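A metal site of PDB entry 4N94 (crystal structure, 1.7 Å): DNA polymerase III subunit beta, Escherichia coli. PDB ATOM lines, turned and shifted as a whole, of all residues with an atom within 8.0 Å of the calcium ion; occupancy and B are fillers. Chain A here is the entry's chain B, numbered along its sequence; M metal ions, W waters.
N of Gly 85 is in hydrogen-bond range of OE2 of Glu 8 (2.9 Å). The side-chain carboxylate of Glu 87 is in hydrogen-bond range of the side-chain amide nitrogen of Gln 61, 2.7 Å away. O of Glu 87 lies within hydrogen-bond range of OG of Ser 101, at 2.7 Å.
The nearest printed residue that does not touch the calcium ion is Ala 86 (4.4 Å).
The calcium ion is bound by the backbone carbonyl oxygen (O) of Gly 85 (2.2 Å). The calcium ion is bound by water W1 (2.3 Å). The calcium ion is bound by OE2 of Glu 87 (2.4 Å). The calcium ion is bound by OE2 of Glu 6, 2.8 Å away.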
ATOM      1  N   VAL A   5     -16.820 -14.595  -2.299  1.00  0.00           N
ATOM      2  CA  VAL A   5     -15.614 -14.149  -3.023  1.00  0.00           C
ATOM      3  C   VAL A   5     -15.866 -14.034  -4.526  1.00  0.00           C
ATOM      4  O   VAL A   5     -16.444 -14.956  -5.145  1.00  0.00           O
ATOM      5  CB  VAL A   5     -14.429 -15.132  -2.828  1.00  0.00           C
ATOM      6  CG1 VAL A   5     -13.177 -14.612  -3.497  1.00  0.00           C
ATOM      7  CG2 VAL A   5     -14.163 -15.406  -1.356  1.00  0.00           C
ATOM      8  N   GLU A   6     -15.397 -12.944  -5.131  1.00  0.00           N
ATOM      9  CA  GLU A   6     -15.493 -12.800  -6.565  1.00  0.00           C
ATOM     10  C   GLU A   6     -14.752 -13.948  -7.253  1.00  0.00           C
ATOM     11  O   GLU A   6     -13.657 -14.335  -6.836  1.00  0.00           O
ATOM     12  CB  GLU A   6     -14.942 -11.435  -7.019  1.00  0.00           C
ATOM     13  CG  GLU A   6     -15.227 -11.152  -8.491  1.00  0.00           C
ATOM     14  CD  GLU A   6     -15.420  -9.678  -8.808  1.00  0.00           C
ATOM     15  OE1 GLU A   6     -14.619  -8.847  -8.300  1.00  0.00           O
ATOM     16  OE2 GLU A   6     -16.394  -9.322  -9.536  1.00  0.00           O
ATOM     17  N   ARG A   7     -15.363 -14.474  -8.299  1.00  0.00           N
ATOM     18  CA  ARG A   7     -14.868 -15.631  -9.032  1.00  0.00           C
ATOM     19  C   ARG A   7     -13.364 -15.627  -9.289  1.00  0.00           C
ATOM     20  O   ARG A   7     -12.678 -16.613  -8.988  1.00  0.00           O
ATOM     21  CB  ARG A   7     -15.585 -15.705 -10.390  1.00  0.00           C
ATOM     22  CG  ARG A   7     -15.058 -16.772 -11.343  1.00  0.00           C
ATOM     23  CD  ARG A   7     -15.946 -16.905 -12.568  1.00  0.00           C
ATOM     24  NE  ARG A   7     -15.436 -17.891 -13.528  1.00  0.00           N
ATOM     25  CZ  ARG A   7     -14.468 -17.654 -14.418  1.00  0.00           C
ATOM     26  NH1 ARG A   7     -13.874 -16.449 -14.512  1.00  0.00           N
ATOM     27  NH2 ARG A   7     -14.085 -18.623 -15.223  1.00  0.00           N
ATOM     28  N   GLU A   8     -12.873 -14.537  -9.890  1.00  0.00           N
ATOM     29  CA  GLU A   8     -11.471 -14.473 -10.316  1.00  0.00           C
ATOM     30  C   GLU A   8     -10.464 -14.394  -9.175  1.00  0.00           C
ATOM     31  O   GLU A   8      -9.268 -14.673  -9.400  1.00  0.00           O
ATOM     32  CB  GLU A   8     -11.242 -13.312 -11.301  1.00  0.00           C
ATOM     33  CG  GLU A   8     -12.018 -13.466 -12.600  1.00  0.00           C
ATOM     34  CD  GLU A   8     -13.498 -13.229 -12.438  1.00  0.00           C
ATOM     35  OE1 GLU A   8     -13.879 -12.373 -11.619  1.00  0.00           O
ATOM     36  OE2 GLU A   8     -14.309 -13.894 -13.105  1.00  0.00           O
ATOM     37  N   GLN A  61     -15.414  -9.335   1.692  1.00  0.00           N
ATOM     38  CA  GLN A  61     -16.860  -9.379   1.924  1.00  0.00           C
ATOM     39  C   GLN A  61     -17.063 -10.026   3.284  1.00  0.00           C
ATOM     40  O   GLN A  61     -16.118 -10.638   3.812  1.00  0.00           O
ATOM     41  CB  GLN A  61     -17.546 -10.164   0.819  1.00  0.00           C
ATOM     42  CG  GLN A  61     -17.360  -9.509  -0.541  1.00  0.00           C
ATOM     43  CD  GLN A  61     -18.232 -10.101  -1.622  1.00  0.00           C
ATOM     44  OE1 GLN A  61     -19.446 -10.217  -1.472  1.00  0.00           O
ATOM     45  NE2 GLN A  61     -17.616 -10.482  -2.730  1.00  0.00           N
ATOM     46  N   PRO A  83     -20.110 -17.243 -14.592  1.00  0.00           N
ATOM     47  CA  PRO A  83     -19.744 -16.190 -15.527  1.00  0.00           C
ATOM     48  C   PRO A  83     -18.738 -15.223 -14.894  1.00  0.00           C
ATOM     49  O   PRO A  83     -18.632 -15.137 -13.679  1.00  0.00           O
ATOM     50  CB  PRO A  83     -21.075 -15.501 -15.815  1.00  0.00           C
ATOM     51  CG  PRO A  83     -21.916 -15.743 -14.606  1.00  0.00           C
ATOM     52  CD  PRO A  83     -21.515 -17.148 -14.176  1.00  0.00           C
ATOM     53  N   GLU A  84     -17.996 -14.524 -15.738  1.00  0.00           N
ATOM     54  CA  GLU A  84     -16.992 -13.612 -15.253  1.00  0.00           C
ATOM     55  C   GLU A  84     -17.568 -12.603 -14.274  1.00  0.00           C
ATOM     56  O   GLU A  84     -18.647 -12.057 -14.473  1.00  0.00           O
ATOM     57  CB  GLU A  84     -16.377 -12.883 -16.418  1.00  0.00           C
ATOM     58  CG  GLU A  84     -15.214 -12.011 -16.038  1.00  0.00           C
ATOM     59  CD  GLU A  84     -14.303 -11.808 -17.206  1.00  0.00           C
ATOM     60  OE1 GLU A  84     -14.803 -11.910 -18.343  1.00  0.00           O
ATOM     61  OE2 GLU A  84     -13.097 -11.559 -16.990  1.00  0.00           O
ATOM     62  N   GLY A  85     -16.818 -12.367 -13.198  1.00  0.00           N
ATOM     63  CA  GLY A  85     -17.231 -11.409 -12.166  1.00  0.00           C
ATOM     64  C   GLY A  85     -18.269 -11.960 -11.183  1.00  0.00           C
ATOM     65  O   GLY A  85     -18.728 -11.246 -10.307  1.00  0.00           O
ATOM     66  N   ALA A  86     -18.646 -13.223 -11.328  1.00  0.00           N
ATOM     67  CA  ALA A  86     -19.649 -13.846 -10.492  1.00  0.00           C
ATOM     68  C   ALA A  86     -19.220 -13.794  -9.019  1.00  0.00           C
ATOM     69  O   ALA A  86     -18.070 -14.114  -8.709  1.00  0.00           O
ATOM     70  CB  ALA A  86     -19.859 -15.301 -10.922  1.00  0.00           C
ATOM     71  N   GLU A  87     -20.150 -13.429  -8.141  1.00  0.00           N
ATOM     72  CA  GLU A  87     -19.960 -13.513  -6.702  1.00  0.00           C
ATOM     73  C   GLU A  87     -20.287 -14.917  -6.234  1.00  0.00           C
ATOM     74  O   GLU A  87     -21.369 -15.399  -6.478  1.00  0.00           O
ATOM     75  CB  GLU A  87     -20.807 -12.499  -5.971  1.00  0.00           C
ATOM     76  CG  GLU A  87     -20.572 -11.078  -6.406  1.00  0.00           C
ATOM     77  CD  GLU A  87     -19.125 -10.643  -6.224  1.00  0.00           C
ATOM     78  OE1 GLU A  87     -18.477 -11.032  -5.231  1.00  0.00           O
ATOM     79  OE2 GLU A  87     -18.656  -9.889  -7.095  1.00  0.00           O
ATOM     80  N   ILE A  88     -19.340 -15.571  -5.581  1.00  0.00           N
ATOM     81  CA  ILE A  88     -19.482 -16.959  -5.184  1.00  0.00           C
ATOM     82  C   ILE A  88     -19.658 -16.998  -3.674  1.00  0.00           C
ATOM     83  O   ILE A  88     -18.677 -16.794  -2.912  1.00  0.00           O
ATOM     84  CB  ILE A  88     -18.286 -17.811  -5.618  1.00  0.00           C
ATOM     85  CG1 ILE A  88     -18.065 -17.675  -7.130  1.00  0.00           C
ATOM     86  CG2 ILE A  88     -18.528 -19.271  -5.305  1.00  0.00           C
ATOM     87  CD1 ILE A  88     -16.865 -18.401  -7.669  1.00  0.00           C
ATOM     88  N   SER A 101     -24.359 -18.627  -6.631  1.00  0.00           N
ATOM     89  CA  SER A 101     -23.989 -17.445  -7.403  1.00  0.00           C
ATOM     90  C   SER A 101     -25.125 -17.179  -8.383  1.00  0.00           C
ATOM     91  O   SER A 101     -25.488 -18.070  -9.116  1.00  0.00           O
ATOM     92  CB  SER A 101     -22.681 -17.684  -8.152  1.00  0.00           C
ATOM     93  OG  SER A 101     -22.308 -16.491  -8.813  1.00  0.00           O
HETATM   94 CA    CA M   1     -19.185  -9.270  -9.403  1.00  0.00          CA
HETATM   95  O   HOH W   1     -21.500  -9.622  -9.339  1.00  0.00           O
